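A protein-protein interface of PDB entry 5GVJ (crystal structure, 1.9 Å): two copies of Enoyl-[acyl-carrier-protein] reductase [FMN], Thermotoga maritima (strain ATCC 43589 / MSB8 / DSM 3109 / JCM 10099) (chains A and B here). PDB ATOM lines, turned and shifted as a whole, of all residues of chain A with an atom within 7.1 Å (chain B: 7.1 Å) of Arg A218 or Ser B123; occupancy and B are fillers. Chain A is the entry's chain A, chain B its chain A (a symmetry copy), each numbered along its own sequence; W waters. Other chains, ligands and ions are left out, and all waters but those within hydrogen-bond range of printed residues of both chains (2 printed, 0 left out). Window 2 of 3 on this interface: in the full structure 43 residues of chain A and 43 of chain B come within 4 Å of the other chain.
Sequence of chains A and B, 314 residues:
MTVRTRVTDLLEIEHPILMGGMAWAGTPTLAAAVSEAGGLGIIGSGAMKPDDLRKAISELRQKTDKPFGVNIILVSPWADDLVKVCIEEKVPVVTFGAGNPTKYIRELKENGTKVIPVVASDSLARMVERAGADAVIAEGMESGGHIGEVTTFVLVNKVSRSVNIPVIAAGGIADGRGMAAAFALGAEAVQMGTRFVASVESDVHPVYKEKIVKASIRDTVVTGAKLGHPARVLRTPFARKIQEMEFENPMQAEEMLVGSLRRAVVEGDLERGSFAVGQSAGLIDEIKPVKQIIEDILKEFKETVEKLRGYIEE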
ATOM      1  N   ALA A 215      12.855   5.685 -17.069  1.00  0.00           N
ATOM      2  CA  ALA A 215      12.022   6.865 -16.883  1.00  0.00           C
ATOM      3  C   ALA A 215      12.256   7.883 -17.993  1.00  0.00           C
ATOM      4  O   ALA A 215      13.391   8.106 -18.420  1.00  0.00           O
ATOM      5  CB  ALA A 215      12.315   7.513 -15.530  1.00  0.00           C
ATOM      6  N   SER A 216      11.170   8.512 -18.449  1.00  0.00           N
ATOM      7  CA  SER A 216      11.235   9.602 -19.414  1.00  0.00           C
ATOM      8  C   SER A 216      11.275  10.950 -18.693  1.00  0.00           C
ATOM      9  O   SER A 216      11.207  11.030 -17.465  1.00  0.00           O
ATOM     10  CB  SER A 216      10.028   9.555 -20.345  1.00  0.00           C
ATOM     11  OG  SER A 216       8.888   9.982 -19.627  1.00  0.00           O
ATOM     12  N   ILE A 217      11.343  12.042 -19.468  1.00  0.00           N
ATOM     13  CA  ILE A 217      11.383  13.371 -18.860  1.00  0.00           C
ATOM     14  C   ILE A 217      10.068  13.726 -18.174  1.00  0.00           C
ATOM     15  O   ILE A 217      10.026  14.672 -17.378  1.00  0.00           O
ATOM     16  CB  ILE A 217      11.754  14.449 -19.902  1.00  0.00           C
ATOM     17  CG1 ILE A 217      10.696  14.518 -21.009  1.00  0.00           C
ATOM     18  CG2 ILE A 217      13.140  14.164 -20.489  1.00  0.00           C
ATOM     19  CD1 ILE A 217      11.011  15.562 -22.087  1.00  0.00           C
ATOM     20  N   ARG A 218       8.992  12.985 -18.454  1.00  0.00           N
ATOM     21  CA  ARG A 218       7.673  13.251 -17.888  1.00  0.00           C
ATOM     22  C   ARG A 218       7.292  12.274 -16.784  1.00  0.00           C
ATOM     23  O   ARG A 218       6.151  12.299 -16.317  1.00  0.00           O
ATOM     24  CB  ARG A 218       6.605  13.208 -18.991  1.00  0.00           C
ATOM     25  CG  ARG A 218       6.640  14.388 -19.938  1.00  0.00           C
ATOM     26  CD  ARG A 218       5.414  14.400 -20.862  1.00  0.00           C
ATOM     27  NE  ARG A 218       5.352  13.184 -21.675  1.00  0.00           N
ATOM     28  CZ  ARG A 218       4.348  12.889 -22.496  1.00  0.00           C
ATOM     29  NH1 ARG A 218       3.325  13.729 -22.613  1.00  0.00           N
ATOM     30  NH2 ARG A 218       4.367  11.761 -23.202  1.00  0.00           N
ATOM     31  N   ASP A 219       8.208  11.410 -16.350  1.00  0.00           N
ATOM     32  CA  ASP A 219       7.847  10.341 -15.432  1.00  0.00           C
ATOM     33  C   ASP A 219       8.097  10.691 -13.972  1.00  0.00           C
ATOM     34  O   ASP A 219       8.156   9.785 -13.136  1.00  0.00           O
ATOM     35  CB  ASP A 219       8.590   9.059 -15.790  1.00  0.00           C
ATOM     36  CG  ASP A 219       7.961   8.336 -16.964  1.00  0.00           C
ATOM     37  OD1 ASP A 219       6.761   8.561 -17.240  1.00  0.00           O
ATOM     38  OD2 ASP A 219       8.672   7.547 -17.609  1.00  0.00           O
ATOM     39  N   THR A 220       8.256  11.967 -13.637  1.00  0.00           N
ATOM     40  CA  THR A 220       8.300  12.338 -12.231  1.00  0.00           C
ATOM     41  C   THR A 220       7.043  13.115 -11.867  1.00  0.00           C
ATOM     42  O   THR A 220       6.335  13.637 -12.732  1.00  0.00           O
ATOM     43  CB  THR A 220       9.552  13.160 -11.885  1.00  0.00           C
ATOM     44  OG1 THR A 220       9.444  14.460 -12.471  1.00  0.00           O
ATOM     45  CG2 THR A 220      10.820  12.473 -12.390  1.00  0.00           C
ATOM     46  N   VAL A 221       6.754  13.152 -10.568  1.00  0.00           N
ATOM     47  CA  VAL A 221       5.634  13.904 -10.013  1.00  0.00           C
ATOM     48  C   VAL A 221       6.135  14.683  -8.820  1.00  0.00           C
ATOM     49  O   VAL A 221       7.081  14.274  -8.143  1.00  0.00           O
ATOM     50  CB  VAL A 221       4.465  13.013  -9.549  1.00  0.00           C
ATOM     51  CG1 VAL A 221       3.551  12.712 -10.668  1.00  0.00           C
ATOM     52  CG2 VAL A 221       4.993  11.740  -8.933  1.00  0.00           C
ATOM     53  N   ARG A 235       7.022   8.481 -10.907  1.00  0.00           N
ATOM     54  CA  ARG A 235       5.591   8.178 -10.914  1.00  0.00           C
ATOM     55  C   ARG A 235       5.324   6.717 -10.559  1.00  0.00           C
ATOM     56  O   ARG A 235       4.898   5.932 -11.410  1.00  0.00           O
ATOM     57  CB  ARG A 235       4.974   8.509 -12.279  1.00  0.00           C
ATOM     58  CG  ARG A 235       4.828  10.001 -12.528  1.00  0.00           C
ATOM     59  CD  ARG A 235       4.027  10.319 -13.795  1.00  0.00           C
ATOM     60  NE  ARG A 235       4.062  11.751 -14.079  1.00  0.00           N
ATOM     61  CZ  ARG A 235       3.060  12.589 -13.830  1.00  0.00           C
ATOM     62  NH1 ARG A 235       1.937  12.137 -13.290  1.00  0.00           N
ATOM     63  NH2 ARG A 235       3.185  13.879 -14.113  1.00  0.00           N
ATOM     64  N   GLN A 279      14.011  15.306 -13.231  1.00  0.00           N
ATOM     65  CA  GLN A 279      13.582  15.187 -14.615  1.00  0.00           C
ATOM     66  C   GLN A 279      14.727  14.772 -15.520  1.00  0.00           C
ATOM     67  O   GLN A 279      14.481  14.231 -16.604  1.00  0.00           O
ATOM     68  CB  GLN A 279      12.965  16.519 -15.097  1.00  0.00           C
ATOM     69  CG  GLN A 279      11.649  16.856 -14.397  1.00  0.00           C
ATOM     70  CD  GLN A 279      10.993  18.114 -14.950  1.00  0.00           C
ATOM     71  OE1 GLN A 279      11.552  18.786 -15.812  1.00  0.00           O
ATOM     72  NE2 GLN A 279       9.796  18.433 -14.452  1.00  0.00           N
ATOM     73  N   GLY A 282      15.056  11.397 -17.657  1.00  0.00           N
ATOM     74  CA  GLY A 282      14.690  11.201 -19.050  1.00  0.00           C
ATOM     75  C   GLY A 282      15.829  11.385 -20.029  1.00  0.00           C
ATOM     76  O   GLY A 282      15.688  11.021 -21.201  1.00  0.00           O
ATOM     77  N   VAL B 119       5.300  22.369 -28.210  1.00  0.00           N
ATOM     78  CA  VAL B 119       5.208  21.063 -27.571  1.00  0.00           C
ATOM     79  C   VAL B 119       5.783  21.158 -26.165  1.00  0.00           C
ATOM     80  O   VAL B 119       6.660  21.979 -25.885  1.00  0.00           O
ATOM     81  CB  VAL B 119       5.934  19.959 -28.372  1.00  0.00           C
ATOM     82  CG1 VAL B 119       5.393  19.884 -29.803  1.00  0.00           C
ATOM     83  CG2 VAL B 119       7.431  20.201 -28.382  1.00  0.00           C
ATOM     84  N   ALA B 120       5.253  20.332 -25.267  1.00  0.00           N
ATOM     85  CA  ALA B 120       5.790  20.211 -23.919  1.00  0.00           C
ATOM     86  C   ALA B 120       6.293  18.800 -23.668  1.00  0.00           C
ATOM     87  O   ALA B 120       6.577  18.431 -22.518  1.00  0.00           O
ATOM     88  CB  ALA B 120       4.734  20.616 -22.884  1.00  0.00           C
ATOM     89  N   SER B 121       6.427  18.002 -24.720  1.00  0.00           N
ATOM     90  CA  SER B 121       6.863  16.634 -24.541  1.00  0.00           C
ATOM     91  C   SER B 121       7.760  16.227 -25.693  1.00  0.00           C
ATOM     92  O   SER B 121       7.719  16.789 -26.788  1.00  0.00           O
ATOM     93  CB  SER B 121       5.678  15.668 -24.437  1.00  0.00           C
ATOM     94  OG  SER B 121       4.971  15.622 -25.665  1.00  0.00           O
ATOM     95  N   ASP B 122       8.567  15.215 -25.406  1.00  0.00           N
ATOM     96  CA  ASP B 122       9.418  14.591 -26.400  1.00  0.00           C
ATOM     97  C   ASP B 122       8.595  13.801 -27.414  1.00  0.00           C
ATOM     98  O   ASP B 122       8.886  13.815 -28.617  1.00  0.00           O
ATOM     99  CB  ASP B 122      10.399  13.684 -25.662  1.00  0.00           C
ATOM    100  CG  ASP B 122      11.360  13.025 -26.577  1.00  0.00           C
ATOM    101  OD1 ASP B 122      11.890  13.718 -27.469  1.00  0.00           O
ATOM    102  OD2 ASP B 122      11.598  11.812 -26.399  1.00  0.00           O
ATOM    103  N   SER B 123       7.565  13.100 -26.942  1.00  0.00           N
ATOM    104  CA  SER B 123       6.753  12.279 -27.834  1.00  0.00           C
ATOM    105  C   SER B 123       5.981  13.146 -28.823  1.00  0.00           C
ATOM    106  O   SER B 123       5.935  12.844 -30.020  1.00  0.00           O
ATOM    107  CB  SER B 123       5.796  11.410 -27.019  1.00  0.00           C
ATOM    108  OG  SER B 123       4.960  12.226 -26.215  1.00  0.00           O
ATOM    109  N   LEU B 124       5.367  14.232 -28.344  1.00  0.00           N
ATOM    110  CA  LEU B 124       4.638  15.101 -29.265  1.00  0.00           C
ATOM    111  C   LEU B 124       5.572  15.690 -30.310  1.00  0.00           C
ATOM    112  O   LEU B 124       5.224  15.753 -31.496  1.00  0.00           O
ATOM    113  CB  LEU B 124       3.901  16.212 -28.511  1.00  0.00           C
ATOM    114  CG  LEU B 124       3.081  17.152 -29.401  1.00  0.00           C
ATOM    115  CD1 LEU B 124       2.061  16.377 -30.232  1.00  0.00           C
ATOM    116  CD2 LEU B 124       2.379  18.254 -28.604  1.00  0.00           C
ATOM    117  N   ALA B 125       6.771  16.110 -29.895  1.00  0.00           N
ATOM    118  CA  ALA B 125       7.736  16.637 -30.856  1.00  0.00           C
ATOM    119  C   ALA B 125       7.999  15.639 -31.974  1.00  0.00           C
ATOM    120  O   ALA B 125       7.956  15.991 -33.159  1.00  0.00           O
ATOM    121  CB  ALA B 125       9.042  17.013 -30.154  1.00  0.00           C
ATOM    122  N   ARG B 126       8.281  14.383 -31.626  1.00  0.00           N
ATOM    123  CA  ARG B 126       8.538  13.404 -32.677  1.00  0.00           C
ATOM    124  C   ARG B 126       7.309  13.187 -33.552  1.00  0.00           C
ATOM    125  O   ARG B 126       7.431  13.007 -34.766  1.00  0.00           O
ATOM    126  CB  ARG B 126       9.006  12.077 -32.087  1.00  0.00           C
ATOM    127  CG  ARG B 126      10.264  12.159 -31.279  1.00  0.00           C
ATOM    128  CD  ARG B 126      10.754  10.753 -31.041  1.00  0.00           C
ATOM    129  NE  ARG B 126       9.978  10.147 -29.970  1.00  0.00           N
ATOM    130  CZ  ARG B 126      10.331  10.163 -28.692  1.00  0.00           C
ATOM    131  NH1 ARG B 126      11.481  10.715 -28.329  1.00  0.00           N
ATOM    132  NH2 ARG B 126       9.542   9.593 -27.783  1.00  0.00           N
ATOM    133  N   MET B 127       6.117  13.207 -32.953  1.00  0.00           N
ATOM    134  CA  MET B 127       4.891  13.033 -33.732  1.00  0.00           C
ATOM    135  C   MET B 127       4.714  14.147 -34.760  1.00  0.00           C
ATOM    136  O   MET B 127       4.411  13.884 -35.931  1.00  0.00           O
ATOM    137  CB  MET B 127       3.687  12.973 -32.793  1.00  0.00           C
ATOM    138  CG  MET B 127       3.697  11.754 -31.865  1.00  0.00           C
ATOM    139  SD  MET B 127       2.130  11.508 -30.997  1.00  0.00           S
ATOM    140  CE  MET B 127       2.142  12.772 -29.743  1.00  0.00           C
ATOM    141  N   VAL B 128       4.898  15.405 -34.346  1.00  0.00           N
ATOM    142  CA  VAL B 128       4.648  16.497 -35.284  1.00  0.00           C
ATOM    143  C   VAL B 128       5.755  16.576 -36.333  1.00  0.00           C
ATOM    144  O   VAL B 128       5.496  16.943 -37.488  1.00  0.00           O
ATOM    145  CB  VAL B 128       4.457  17.835 -34.540  1.00  0.00           C
ATOM    146  CG1 VAL B 128       3.273  17.755 -33.578  1.00  0.00           C
ATOM    147  CG2 VAL B 128       5.709  18.226 -33.793  1.00  0.00           C
ATOM    148  N   GLU B 129       6.993  16.205 -35.976  1.00  0.00           N
ATOM    149  CA  GLU B 129       8.024  16.054 -37.003  1.00  0.00           C
ATOM    150  C   GLU B 129       7.576  15.071 -38.078  1.00  0.00           C
ATOM    151  O   GLU B 129       7.672  15.359 -39.278  1.00  0.00           O
ATOM    152  CB  GLU B 129       9.355  15.591 -36.401  1.00  0.00           C
ATOM    153  CG  GLU B 129      10.437  15.491 -37.468  1.00  0.00           C
ATOM    154  CD  GLU B 129      11.793  15.064 -36.953  1.00  0.00           C
ATOM    155  OE1 GLU B 129      12.810  15.646 -37.386  1.00  0.00           O
ATOM    156  OE2 GLU B 129      11.845  14.140 -36.132  1.00  0.00           O
ATOM    157  N   ARG B 130       7.086  13.899 -37.657  1.00  0.00           N
ATOM    158  CA  ARG B 130       6.631  12.881 -38.605  1.00  0.00           C
ATOM    159  C   ARG B 130       5.538  13.424 -39.517  1.00  0.00           C
ATOM    160  O   ARG B 130       5.525  13.146 -40.723  1.00  0.00           O
ATOM    161  CB  ARG B 130       6.120  11.657 -37.841  1.00  0.00           C
ATOM    162  CG  ARG B 130       7.011  10.429 -37.909  1.00  0.00           C
ATOM    163  CD  ARG B 130       6.412   9.240 -37.142  1.00  0.00           C
ATOM    164  NE  ARG B 130       6.811   9.221 -35.732  1.00  0.00           N
ATOM    165  CZ  ARG B 130       5.969   9.344 -34.705  1.00  0.00           C
ATOM    166  NH1 ARG B 130       4.660   9.481 -34.921  1.00  0.00           N
ATOM    167  NH2 ARG B 130       6.435   9.327 -33.458  1.00  0.00           N
ATOM    168  N   GLU B 149       4.693  19.934 -18.024  1.00  0.00           N
ATOM    169  CA  GLU B 149       5.323  19.488 -16.794  1.00  0.00           C
ATOM    170  C   GLU B 149       6.839  19.591 -16.809  1.00  0.00           C
ATOM    171  O   GLU B 149       7.447  19.639 -15.733  1.00  0.00           O
ATOM    172  CB  GLU B 149       4.937  18.032 -16.504  1.00  0.00           C
ATOM    173  CG  GLU B 149       3.517  17.694 -16.898  1.00  0.00           C
ATOM    174  CD  GLU B 149       3.006  16.448 -16.202  1.00  0.00           C
ATOM    175  OE1 GLU B 149       3.366  15.329 -16.644  1.00  0.00           O
ATOM    176  OE2 GLU B 149       2.256  16.597 -15.207  1.00  0.00           O
ATOM    177  N   VAL B 150       7.462  19.631 -17.985  1.00  0.00           N
ATOM    178  CA  VAL B 150       8.918  19.575 -18.101  1.00  0.00           C
ATOM    179  C   VAL B 150       9.484  20.991 -18.144  1.00  0.00           C
ATOM    180  O   VAL B 150       8.910  21.886 -18.782  1.00  0.00           O
ATOM    181  CB  VAL B 150       9.324  18.772 -19.350  1.00  0.00           C
ATOM    182  CG1 VAL B 150      10.835  18.509 -19.347  1.00  0.00           C
ATOM    183  CG2 VAL B 150       8.548  17.458 -19.407  1.00  0.00           C
ATOM    184  N   VAL B 154      15.602  20.741 -19.229  1.00  0.00           N
ATOM    185  CA  VAL B 154      15.507  19.337 -19.605  1.00  0.00           C
ATOM    186  C   VAL B 154      14.866  19.186 -20.983  1.00  0.00           C
ATOM    187  O   VAL B 154      15.337  18.420 -21.836  1.00  0.00           O
ATOM    188  CB  VAL B 154      14.711  18.575 -18.530  1.00  0.00           C
ATOM    189  CG1 VAL B 154      14.376  17.164 -19.010  1.00  0.00           C
ATOM    190  CG2 VAL B 154      15.492  18.534 -17.195  1.00  0.00           C
ATOM    191  N   LEU B 155      13.767  19.899 -21.210  1.00  0.00           N
ATOM    192  CA  LEU B 155      12.947  19.659 -22.394  1.00  0.00           C
ATOM    193  C   LEU B 155      13.695  19.983 -23.681  1.00  0.00           C
ATOM    194  O   LEU B 155      13.670  19.203 -24.639  1.00  0.00           O
ATOM    195  CB  LEU B 155      11.669  20.483 -22.305  1.00  0.00           C
ATOM    196  CG  LEU B 155      10.703  20.297 -23.471  1.00  0.00           C
ATOM    197  CD1 LEU B 155      10.050  18.921 -23.406  1.00  0.00           C
ATOM    198  CD2 LEU B 155       9.658  21.412 -23.415  1.00  0.00           C
ATOM    199  N   LYS B 158      16.246  17.190 -24.471  1.00  0.00           N
ATOM    200  CA  LYS B 158      15.713  15.916 -24.950  1.00  0.00           C
ATOM    201  C   LYS B 158      15.066  16.074 -26.318  1.00  0.00           C
ATOM    202  O   LYS B 158      15.269  15.243 -27.209  1.00  0.00           O
ATOM    203  CB  LYS B 158      14.703  15.354 -23.948  1.00  0.00           C
ATOM    204  CG  LYS B 158      14.034  14.053 -24.391  1.00  0.00           C
ATOM    205  CD  LYS B 158      15.068  12.938 -24.581  1.00  0.00           C
ATOM    206  CE  LYS B 158      14.401  11.574 -24.725  1.00  0.00           C
ATOM    207  NZ  LYS B 158      15.324  10.560 -25.316  1.00  0.00           N
ATOM    208  N   VAL B 159      14.299  17.145 -26.508  1.00  0.00           N
ATOM    209  CA  VAL B 159      13.604  17.346 -27.779  1.00  0.00           C
ATOM    210  C   VAL B 159      14.606  17.506 -28.915  1.00  0.00           C
ATOM    211  O   VAL B 159      14.477  16.872 -29.966  1.00  0.00           O
ATOM    212  CB  VAL B 159      12.647  18.547 -27.684  1.00  0.00           C
ATOM    213  CG1 VAL B 159      12.142  18.965 -29.069  1.00  0.00           C
ATOM    214  CG2 VAL B 159      11.465  18.206 -26.791  1.00  0.00           C
ATOM    215  N   SER B 162      15.918  14.379 -30.137  1.00  0.00           N
ATOM    216  CA  SER B 162      14.947  13.447 -30.702  1.00  0.00           C
ATOM    217  C   SER B 162      14.529  13.765 -32.130  1.00  0.00           C
ATOM    218  O   SER B 162      14.020  12.869 -32.808  1.00  0.00           O
ATOM    219  CB  SER B 162      13.676  13.409 -29.857  1.00  0.00           C
ATOM    220  OG  SER B 162      13.923  12.934 -28.555  1.00  0.00           O
HETATM  221  O   HOH W   1      17.116  10.337 -23.168  1.00  0.00           O
HETATM  222  O   HOH W   2       7.886  12.950 -23.274  1.00  0.00           O
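Water W1 lies within hydrogen-bond range of O of Gly A282 (2.5 Å) and NZ of Lys B158 (2.8 Å).
Water W2 lies within hydrogen-bond range of NE of Arg A218 and N of Asp B122.
Along chain B the printed residues that touch a printed residue of chain A span positions 121 to 158.
Of the 10 printed residues of chain A, 5 touch a printed residue of chain B.
Printed residues of chain A that touch a printed residue of chain B: Ile A217, Arg A218, Arg A235, Gln A279 and Gly A282.
Among the printed residues, 12 pairs touch across the chains.
Among the printed residues, Asp or Glu carboxylates within 4 Å of a Lys or Arg side-chain nitrogen of the other chain: Arg A235 with Glu B149.
Of chain B, only Ser B121, Ser B123 and Val B150 come within 4 Å of Arg A218.
Of chain A, only Arg A218 (3.1 Å) comes within 4 Å of Ser B123.
Of the printed residues of chain B, Gln A279 touches Glu B149 (2.9 Å), Val B150 (3.6 Å) and Val B154 (3.8 Å).
Printed residues of chain A within 4 Å of Lys B158: Ile A217 (3.98 Å) and Gly A282 (3.8 Å).
Printed residues of chain A within 4 Å of Leu B155: Ile A217 (3.7 Å).
Of the printed residues of chain B, Ile A217 touches Val B150 (3.8 Å), Val B154 (3.6 Å), Leu B155 (3.7 Å) and Lys B158 (3.98 Å).
Printed residues of chain B within 4 Å of Arg A235: Glu B149 (2.9 Å).
The nearest residue of chain A that does not touch Ser B123 is Ile A217 (6.4 Å).
The nearest printed residue of chain B that does not touch Arg A235 is Val B150 (8.1 Å).
NH2 of Arg A218 lies within hydrogen-bond range of OG of Ser B123 (3.1 Å).
NH2 of Arg A235 lies within salt-bridge range of OE1 of Glu B149, 2.9 Å away.
NE2 of Gln A279 lies within hydrogen-bond range of O of Glu B149 (2.9 Å).
Val B150 touches Ile A217 (CG2 to O, 3.8 Å).
Val B154 touches Ile A217.
Ile A217 touches Leu B155.
Ile A217 touches Lys B158.
CB of Ser B121 touches NH1 of Arg A218 (3.6 Å).
Arg A218 touches Val B150 (CG to CG2, 3.7 Å).
Val B150 touches Gln A279 (CA to OE1, 3.6 Å).
Gln A279 touches Val B154.
Gly A282 touches Lys B158.
No position is printed for both chains.
O of Thr A220 lies within hydrogen-bond range of NE of Arg A235 (3.2 Å).
The backbone carbonyl oxygen of Arg A218 is in hydrogen-bond range of the guanidinium group of Arg A235, 3.1 Å away.
The side-chain hydroxyl of Ser B162 lies within hydrogen-bond range of the backbone carbonyl oxygen of Lys B158, at 3.0 Å.
O of Asp A219 is in hydrogen-bond range of N of Arg A235.
The side-chain hydroxyl (OG) of Ser B121 is in hydrogen-bond range of the backbone NH (N) of Leu B124, 3.0 Å away.
The side-chain hydroxyl of Ser B123 sits at hydrogen-bond distance from the side-chain hydroxyl of Ser B121, 3.4 Å away.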
